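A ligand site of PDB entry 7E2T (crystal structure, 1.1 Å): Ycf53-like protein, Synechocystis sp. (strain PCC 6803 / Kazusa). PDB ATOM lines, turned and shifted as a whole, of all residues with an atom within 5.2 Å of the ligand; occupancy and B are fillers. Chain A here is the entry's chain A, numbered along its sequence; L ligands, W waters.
The backbone carbonyl oxygen (O) of Trp 178 lies within hydrogen-bond range of the backbone NH (N) of Trp 183.
OD1 of Asn 211 lies within hydrogen-bond range of N of Leu 213 (3.0 Å).
NE2 of Gln 212 sits at hydrogen-bond distance from O of Leu 210, at 3.1 Å.
OD2 of Asp 109 lies within salt-bridge range of NH1 of Arg 113 (3.0 Å).
The backbone carbonyl oxygen of Trp 183 sits at hydrogen-bond distance from the backbone NH of Thr 190, 3.0 Å away.
An oxygen (O1) of the ligand sits close to the backbone carbonyl oxygen (O) of Thr 190.
Arg 113 touches the ligand (NH1 to C30, 3.2 Å).
O of Trp 183 touches C18 of the ligand, 3.2 Å away.
Trp 189 touches the ligand (CE3 to C22, 3.4 Å).
Trp 192 touches the ligand.
Phe 196 touches the ligand.
Leu 210 touches the ligand (O to C31, 3.6 Å).
Hydrophobic or aromatic side chains within 4 Å of the ligand: Trp 183, Trp 189, Trp 192, Phe 196 and Leu 213.
Of the 17 residues printed, 11 come within 4 Å of the ligand.
The nearest printed residue that does not touch the ligand is Leu 209 (4.1 Å).
Water W1 lies within hydrogen-bond range of O2 of the ligand (2.4 Å) and NH1 of Arg 214 (3.1 Å).
Water W4 lies within hydrogen-bond range of N1 of the ligand (2.9 Å) and N of Trp 192 (3.3 Å).
N of Gln 212 lies within hydrogen-bond range of O6 of the ligand (3.0 Å).
An oxygen (O4) of the ligand is in hydrogen-bond range of the side-chain amide nitrogen (ND2) of Asn 211, 2.9 Å away.
NH2 of Arg 214 is in salt-bridge range of O4 of the ligand (3.0 Å).
O6 of the ligand sits at hydrogen-bond distance from N of Leu 213 (3.5 Å).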
ATOM      1  N   ASP A 109       9.896  -2.707  -4.697  1.00  0.00           N
ATOM      2  CA  ASP A 109      10.722  -3.473  -3.768  1.00  0.00           C
ATOM      3  C   ASP A 109       9.939  -3.841  -2.519  1.00  0.00           C
ATOM      4  O   ASP A 109      10.017  -4.971  -2.034  1.00  0.00           O
ATOM      5  CB  ASP A 109      11.958  -2.638  -3.426  1.00  0.00           C
ATOM      6  CG  ASP A 109      12.961  -3.413  -2.613  1.00  0.00           C
ATOM      7  OD1 ASP A 109      13.478  -4.417  -3.171  1.00  0.00           O
ATOM      8  OD2 ASP A 109      13.224  -3.021  -1.458  1.00  0.00           O
ATOM      9  N   ARG A 113       8.925  -7.757  -1.332  1.00  0.00           N
ATOM     10  CA  ARG A 113       9.276  -8.320  -0.032  1.00  0.00           C
ATOM     11  C   ARG A 113       8.019  -8.875   0.634  1.00  0.00           C
ATOM     12  O   ARG A 113       8.035  -9.984   1.198  1.00  0.00           O
ATOM     13  CB  ARG A 113       9.956  -7.235   0.802  1.00  0.00           C
ATOM     14  CG  ARG A 113      10.410  -7.642   2.186  1.00  0.00           C
ATOM     15  CD  ARG A 113      11.475  -6.694   2.758  1.00  0.00           C
ATOM     16  NE  ARG A 113      11.122  -5.286   2.642  1.00  0.00           N
ATOM     17  CZ  ARG A 113      11.621  -4.442   1.740  1.00  0.00           C
ATOM     18  NH1 ARG A 113      12.552  -4.825   0.869  1.00  0.00           N
ATOM     19  NH2 ARG A 113      11.215  -3.192   1.738  1.00  0.00           N
ATOM     20  N   GLN A 128       7.461 -11.572   9.339  1.00  0.00           N
ATOM     21  CA  GLN A 128       7.902 -10.553   8.383  1.00  0.00           C
ATOM     22  C   GLN A 128       9.353 -10.741   7.953  1.00  0.00           C
ATOM     23  O   GLN A 128      10.031  -9.756   7.628  1.00  0.00           O
ATOM     24  CB  GLN A 128       7.710  -9.123   8.926  1.00  0.00           C
ATOM     25  CG  GLN A 128       6.333  -8.790   9.444  1.00  0.00           C
ATOM     26  CD  GLN A 128       6.225  -7.350   9.910  1.00  0.00           C
ATOM     27  OE1 GLN A 128       7.202  -6.747  10.381  1.00  0.00           O
ATOM     28  NE2 GLN A 128       5.037  -6.775   9.784  1.00  0.00           N
ATOM     29  N   TRP A 129       9.828 -11.978   7.946  1.00  0.00           N
ATOM     30  CA  TRP A 129      11.130 -12.324   7.379  1.00  0.00           C
ATOM     31  C   TRP A 129      11.116 -13.814   7.092  1.00  0.00           C
ATOM     32  O   TRP A 129      10.285 -14.549   7.628  1.00  0.00           O
ATOM     33  CB  TRP A 129      12.293 -11.887   8.261  1.00  0.00           C
ATOM     34  CG  TRP A 129      12.152 -12.143   9.733  1.00  0.00           C
ATOM     35  CD1 TRP A 129      11.517 -11.345  10.645  1.00  0.00           C
ATOM     36  CD2 TRP A 129      12.671 -13.256  10.449  1.00  0.00           C
ATOM     37  NE1 TRP A 129      11.611 -11.907  11.901  1.00  0.00           N
ATOM     38  CE2 TRP A 129      12.314 -13.079  11.806  1.00  0.00           C
ATOM     39  CE3 TRP A 129      13.393 -14.397  10.095  1.00  0.00           C
ATOM     40  CZ2 TRP A 129      12.654 -13.996  12.805  1.00  0.00           C
ATOM     41  CZ3 TRP A 129      13.753 -15.304  11.083  1.00  0.00           C
ATOM     42  CH2 TRP A 129      13.381 -15.093  12.424  1.00  0.00           C
ATOM     43  N   TRP A 178      28.439  -7.818  -3.054  1.00  0.00           N
ATOM     44  CA  TRP A 178      27.808  -6.626  -2.494  1.00  0.00           C
ATOM     45  C   TRP A 178      28.304  -5.342  -3.133  1.00  0.00           C
ATOM     46  O   TRP A 178      27.478  -4.487  -3.492  1.00  0.00           O
ATOM     47  CB  TRP A 178      28.000  -6.569  -0.988  1.00  0.00           C
ATOM     48  CG  TRP A 178      27.634  -7.768  -0.214  1.00  0.00           C
ATOM     49  CD1 TRP A 178      28.321  -8.258   0.840  1.00  0.00           C
ATOM     50  CD2 TRP A 178      26.504  -8.620  -0.397  1.00  0.00           C
ATOM     51  NE1 TRP A 178      27.708  -9.363   1.337  1.00  0.00           N
ATOM     52  CE2 TRP A 178      26.589  -9.615   0.595  1.00  0.00           C
ATOM     53  CE3 TRP A 178      25.445  -8.670  -1.315  1.00  0.00           C
ATOM     54  CZ2 TRP A 178      25.647 -10.638   0.708  1.00  0.00           C
ATOM     55  CZ3 TRP A 178      24.509  -9.677  -1.196  1.00  0.00           C
ATOM     56  CH2 TRP A 178      24.620 -10.650  -0.190  1.00  0.00           C
ATOM     57  N   TRP A 183      25.428  -2.625  -2.600  1.00  0.00           N
ATOM     58  CA  TRP A 183      24.904  -2.853  -1.256  1.00  0.00           C
ATOM     59  C   TRP A 183      25.952  -2.639  -0.172  1.00  0.00           C
ATOM     60  O   TRP A 183      25.597  -2.563   1.009  1.00  0.00           O
ATOM     61  CB  TRP A 183      24.314  -4.257  -1.127  1.00  0.00           C
ATOM     62  CG  TRP A 183      23.095  -4.494  -1.970  1.00  0.00           C
ATOM     63  CD1 TRP A 183      22.541  -3.647  -2.897  1.00  0.00           C
ATOM     64  CD2 TRP A 183      22.296  -5.684  -1.997  1.00  0.00           C
ATOM     65  NE1 TRP A 183      21.449  -4.235  -3.481  1.00  0.00           N
ATOM     66  CE2 TRP A 183      21.290  -5.486  -2.956  1.00  0.00           C
ATOM     67  CE3 TRP A 183      22.350  -6.907  -1.324  1.00  0.00           C
ATOM     68  CZ2 TRP A 183      20.343  -6.454  -3.253  1.00  0.00           C
ATOM     69  CZ3 TRP A 183      21.414  -7.866  -1.620  1.00  0.00           C
ATOM     70  CH2 TRP A 183      20.431  -7.639  -2.578  1.00  0.00           C
ATOM     71  N   TRP A 189      28.018  -0.537   4.826  1.00  0.00           N
ATOM     72  CA  TRP A 189      26.792  -1.110   4.284  1.00  0.00           C
ATOM     73  C   TRP A 189      25.855   0.023   3.832  1.00  0.00           C
ATOM     74  O   TRP A 189      25.671   1.008   4.535  1.00  0.00           O
ATOM     75  CB  TRP A 189      26.090  -1.948   5.336  1.00  0.00           C
ATOM     76  CG  TRP A 189      26.867  -3.138   5.803  1.00  0.00           C
ATOM     77  CD1 TRP A 189      27.685  -3.213   6.899  1.00  0.00           C
ATOM     78  CD2 TRP A 189      26.878  -4.439   5.205  1.00  0.00           C
ATOM     79  NE1 TRP A 189      28.198  -4.479   7.025  1.00  0.00           N
ATOM     80  CE2 TRP A 189      27.721  -5.257   6.000  1.00  0.00           C
ATOM     81  CE3 TRP A 189      26.279  -4.997   4.073  1.00  0.00           C
ATOM     82  CZ2 TRP A 189      27.966  -6.596   5.692  1.00  0.00           C
ATOM     83  CZ3 TRP A 189      26.510  -6.317   3.783  1.00  0.00           C
ATOM     84  CH2 TRP A 189      27.350  -7.107   4.596  1.00  0.00           C
ATOM     85  N   THR A 190      25.242  -0.152   2.672  1.00  0.00           N
ATOM     86  CA  THR A 190      24.277   0.837   2.203  1.00  0.00           C
ATOM     87  C   THR A 190      23.076   0.811   3.131  1.00  0.00           C
ATOM     88  O   THR A 190      22.473  -0.249   3.363  1.00  0.00           O
ATOM     89  CB  THR A 190      23.877   0.490   0.778  1.00  0.00           C
ATOM     90  OG1 THR A 190      25.080   0.426   0.003  1.00  0.00           O
ATOM     91  CG2 THR A 190      22.963   1.550   0.204  1.00  0.00           C
ATOM     92  N   ARG A 191      22.706   1.978   3.648  1.00  0.00           N
ATOM     93  CA  ARG A 191      21.698   2.036   4.695  1.00  0.00           C
ATOM     94  C   ARG A 191      20.301   1.997   4.102  1.00  0.00           C
ATOM     95  O   ARG A 191      19.993   2.751   3.174  1.00  0.00           O
ATOM     96  CB  ARG A 191      21.848   3.324   5.512  1.00  0.00           C
ATOM     97  N   TRP A 192      19.458   1.120   4.633  1.00  0.00           N
ATOM     98  CA  TRP A 192      18.101   1.018   4.108  1.00  0.00           C
ATOM     99  C   TRP A 192      17.155   1.965   4.852  1.00  0.00           C
ATOM    100  O   TRP A 192      17.193   2.030   6.081  1.00  0.00           O
ATOM    101  CB  TRP A 192      17.575  -0.396   4.285  1.00  0.00           C
ATOM    102  CG  TRP A 192      16.174  -0.539   3.821  1.00  0.00           C
ATOM    103  CD1 TRP A 192      15.769  -0.756   2.557  1.00  0.00           C
ATOM    104  CD2 TRP A 192      14.993  -0.459   4.614  1.00  0.00           C
ATOM    105  NE1 TRP A 192      14.400  -0.830   2.489  1.00  0.00           N
ATOM    106  CE2 TRP A 192      13.901  -0.641   3.749  1.00  0.00           C
ATOM    107  CE3 TRP A 192      14.747  -0.244   5.971  1.00  0.00           C
ATOM    108  CZ2 TRP A 192      12.583  -0.620   4.201  1.00  0.00           C
ATOM    109  CZ3 TRP A 192      13.437  -0.222   6.412  1.00  0.00           C
ATOM    110  CH2 TRP A 192      12.371  -0.416   5.530  1.00  0.00           C
ATOM    111  N   PHE A 196      19.822   3.672  -0.778  1.00  0.00           N
ATOM    112  CA  PHE A 196      19.652   2.957  -2.028  1.00  0.00           C
ATOM    113  C   PHE A 196      19.236   3.907  -3.161  1.00  0.00           C
ATOM    114  O   PHE A 196      18.771   5.024  -2.926  1.00  0.00           O
ATOM    115  CB  PHE A 196      18.676   1.801  -1.811  1.00  0.00           C
ATOM    116  CG  PHE A 196      19.273   0.726  -0.953  1.00  0.00           C
ATOM    117  CD1 PHE A 196      20.026  -0.257  -1.526  1.00  0.00           C
ATOM    118  CD2 PHE A 196      19.192   0.777   0.415  1.00  0.00           C
ATOM    119  CE1 PHE A 196      20.637  -1.221  -0.762  1.00  0.00           C
ATOM    120  CE2 PHE A 196      19.806  -0.180   1.191  1.00  0.00           C
ATOM    121  CZ  PHE A 196      20.529  -1.179   0.594  1.00  0.00           C
ATOM    122  N   LEU A 209      15.938  -5.816  -3.155  1.00  0.00           N
ATOM    123  CA  LEU A 209      16.823  -5.930  -2.012  1.00  0.00           C
ATOM    124  C   LEU A 209      16.598  -7.230  -1.248  1.00  0.00           C
ATOM    125  O   LEU A 209      15.475  -7.721  -1.124  1.00  0.00           O
ATOM    126  CB  LEU A 209      16.589  -4.773  -1.045  1.00  0.00           C
ATOM    127  CG  LEU A 209      16.882  -3.388  -1.625  1.00  0.00           C
ATOM    128  CD1 LEU A 209      16.743  -2.339  -0.525  1.00  0.00           C
ATOM    129  CD2 LEU A 209      18.249  -3.299  -2.296  1.00  0.00           C
ATOM    130  N   LEU A 210      17.683  -7.756  -0.678  1.00  0.00           N
ATOM    131  CA  LEU A 210      17.698  -8.904   0.221  1.00  0.00           C
ATOM    132  C   LEU A 210      18.488  -8.483   1.459  1.00  0.00           C
ATOM    133  O   LEU A 210      19.718  -8.475   1.450  1.00  0.00           O
ATOM    134  CB  LEU A 210      18.315 -10.116  -0.451  1.00  0.00           C
ATOM    135  CG  LEU A 210      17.566 -10.648  -1.669  1.00  0.00           C
ATOM    136  CD1 LEU A 210      18.417 -11.615  -2.468  1.00  0.00           C
ATOM    137  CD2 LEU A 210      16.247 -11.329  -1.240  1.00  0.00           C
ATOM    138  N   ASN A 211      17.787  -8.135   2.527  1.00  0.00           N
ATOM    139  CA  ASN A 211      18.451  -7.732   3.766  1.00  0.00           C
ATOM    140  C   ASN A 211      19.439  -8.789   4.228  1.00  0.00           C
ATOM    141  O   ASN A 211      19.144  -9.985   4.201  1.00  0.00           O
ATOM    142  CB  ASN A 211      17.357  -7.525   4.815  1.00  0.00           C
ATOM    143  CG  ASN A 211      17.855  -6.874   6.103  1.00  0.00           C
ATOM    144  OD1 ASN A 211      19.032  -6.491   6.214  1.00  0.00           O
ATOM    145  ND2 ASN A 211      16.972  -6.767   7.081  1.00  0.00           N
ATOM    146  N   GLN A 212      20.637  -8.349   4.619  1.00  0.00           N
ATOM    147  CA  GLN A 212      21.681  -9.233   5.124  1.00  0.00           C
ATOM    148  C   GLN A 212      21.738  -9.281   6.650  1.00  0.00           C
ATOM    149  O   GLN A 212      22.653  -9.907   7.188  1.00  0.00           O
ATOM    150  CB  GLN A 212      23.032  -8.842   4.531  1.00  0.00           C
ATOM    151  CG  GLN A 212      23.081  -9.098   3.039  1.00  0.00           C
ATOM    152  CD  GLN A 212      22.775 -10.549   2.702  1.00  0.00           C
ATOM    153  OE1 GLN A 212      23.475 -11.453   3.148  1.00  0.00           O
ATOM    154  NE2 GLN A 212      21.680 -10.785   1.962  1.00  0.00           N
ATOM    155  N   LEU A 213      20.759  -8.691   7.352  1.00  0.00           N
ATOM    156  CA  LEU A 213      20.752  -8.679   8.809  1.00  0.00           C
ATOM    157  C   LEU A 213      20.768 -10.087   9.399  1.00  0.00           C
ATOM    158  O   LEU A 213      21.305 -10.279  10.492  1.00  0.00           O
ATOM    159  CB  LEU A 213      19.514  -7.949   9.310  1.00  0.00           C
ATOM    160  CG  LEU A 213      19.266  -7.817  10.809  1.00  0.00           C
ATOM    161  CD1 LEU A 213      20.396  -7.013  11.424  1.00  0.00           C
ATOM    162  CD2 LEU A 213      17.918  -7.167  11.049  1.00  0.00           C
ATOM    163  N   ARG A 214      20.167 -11.063   8.732  1.00  0.00           N
ATOM    164  CA  ARG A 214      20.169 -12.440   9.190  1.00  0.00           C
ATOM    165  C   ARG A 214      21.049 -13.317   8.295  1.00  0.00           C
ATOM    166  O   ARG A 214      20.813 -14.527   8.178  1.00  0.00           O
ATOM    167  CB  ARG A 214      18.737 -12.978   9.260  1.00  0.00           C
ATOM    168  CG  ARG A 214      17.960 -12.371  10.421  1.00  0.00           C
ATOM    169  CD  ARG A 214      16.438 -12.576  10.268  1.00  0.00           C
ATOM    170  NE  ARG A 214      15.969 -11.808   9.121  1.00  0.00           N
ATOM    171  CZ  ARG A 214      15.444 -10.591   9.178  1.00  0.00           C
ATOM    172  NH1 ARG A 214      15.262  -9.982  10.336  1.00  0.00           N
ATOM    173  NH2 ARG A 214      15.119  -9.982   8.054  1.00  0.00           N
HETATM  174  N1  LIG L   1      20.146  -3.379   4.634  1.00  0.00           N
HETATM  175  O1  LIG L   1      22.514  -2.993   5.002  1.00  0.00           O
HETATM  176  N2  LIG L   1      18.686  -3.724   8.346  1.00  0.00           N
HETATM  177  C1  LIG L   1      16.184  -3.718   6.606  1.00  0.00           C
HETATM  178  C2  LIG L   1      19.413  -3.960   3.433  1.00  0.00           C
HETATM  179  C3  LIG L   1      22.333  -5.429   6.608  1.00  0.00           C
HETATM  180  C4  LIG L   1      19.408  -3.618   9.485  1.00  0.00           C
HETATM  181  C5  LIG L   1      15.096  -3.966   5.577  1.00  0.00           C
HETATM  182  C6  LIG L   1      20.450  -4.288   2.436  1.00  0.00           C
HETATM  183  C7  LIG L   1      23.592  -5.048   7.255  1.00  0.00           C
HETATM  184  C8  LIG L   1      18.537  -3.384  10.537  1.00  0.00           C
HETATM  185  C9  LIG L   1      15.703  -4.143   4.257  1.00  0.00           C
HETATM  186  C10 LIG L   1      21.736  -3.957   2.937  1.00  0.00           C
HETATM  187  C11 LIG L   1      23.237  -4.222   8.489  1.00  0.00           C
HETATM  188  C12 LIG L   1      17.288  -3.335  10.038  1.00  0.00           C
HETATM  189  C13 LIG L   1      17.158  -4.014   4.405  1.00  0.00           C
HETATM  190  C14 LIG L   1      21.635  -3.382   4.305  1.00  0.00           C
HETATM  191  C15 LIG L   1      21.670  -4.182   8.540  1.00  0.00           C
HETATM  192  C16 LIG L   1      17.392  -3.555   8.671  1.00  0.00           C
HETATM  193  C17 LIG L   1      13.589  -4.020   5.869  1.00  0.00           C
HETATM  194  C18 LIG L   1      23.048  -4.154   2.179  1.00  0.00           C
HETATM  195  C19 LIG L   1      24.077  -3.451   9.140  1.00  0.00           C
HETATM  196  C20 LIG L   1      16.025  -3.079  10.876  1.00  0.00           C
HETATM  197  C21 LIG L   1      13.150  -5.491   5.839  1.00  0.00           C
HETATM  198  C22 LIG L   1      23.444  -5.641   2.230  1.00  0.00           C
HETATM  199  C23 LIG L   1      23.800  -2.950  10.563  1.00  0.00           C
HETATM  200  C24 LIG L   1      15.500  -4.412  11.408  1.00  0.00           C
HETATM  201  C25 LIG L   1      13.690  -6.255   7.058  1.00  0.00           C
HETATM  202  C26 LIG L   1      14.209  -4.250  12.206  1.00  0.00           C
HETATM  203  C27 LIG L   1      16.062  -3.540   7.902  1.00  0.00           C
HETATM  204  C28 LIG L   1      18.127  -4.144   3.249  1.00  0.00           C
HETATM  205  C29 LIG L   1      20.937  -3.751   9.575  1.00  0.00           C
HETATM  206  C30 LIG L   1      14.992  -4.399   2.934  1.00  0.00           C
HETATM  207  C31 LIG L   1      20.143  -4.884   1.076  1.00  0.00           C
HETATM  208  C32 LIG L   1      24.424  -6.274   7.654  1.00  0.00           C
HETATM  209  C33 LIG L   1      18.903  -3.191  12.019  1.00  0.00           C
HETATM  210  N3  LIG L   1      17.478  -3.774   5.811  1.00  0.00           N
HETATM  211  N4  LIG L   1      21.193  -4.898   7.378  1.00  0.00           N
HETATM  212  O2  LIG L   1      13.643  -5.740   8.212  1.00  0.00           O
HETATM  213  O3  LIG L   1      13.760  -3.112  12.517  1.00  0.00           O
HETATM  214  O4  LIG L   1      14.196  -7.400   6.905  1.00  0.00           O
HETATM  215  O5  LIG L   1      13.596  -5.294  12.566  1.00  0.00           O
HETATM  216  O6  LIG L   1      22.212  -6.063   5.618  1.00  0.00           O
HETATM  217  O   HOH W   1      13.735  -7.286  10.048  1.00  0.00           O
HETATM  218  O   HOH W   2      22.709  -0.986   6.804  1.00  0.00           O
HETATM  219  O   HOH W   3      13.641  -9.030   4.982  1.00  0.00           O
HETATM  220  O   HOH W   4      19.885  -1.398   6.720  1.00  0.00           O
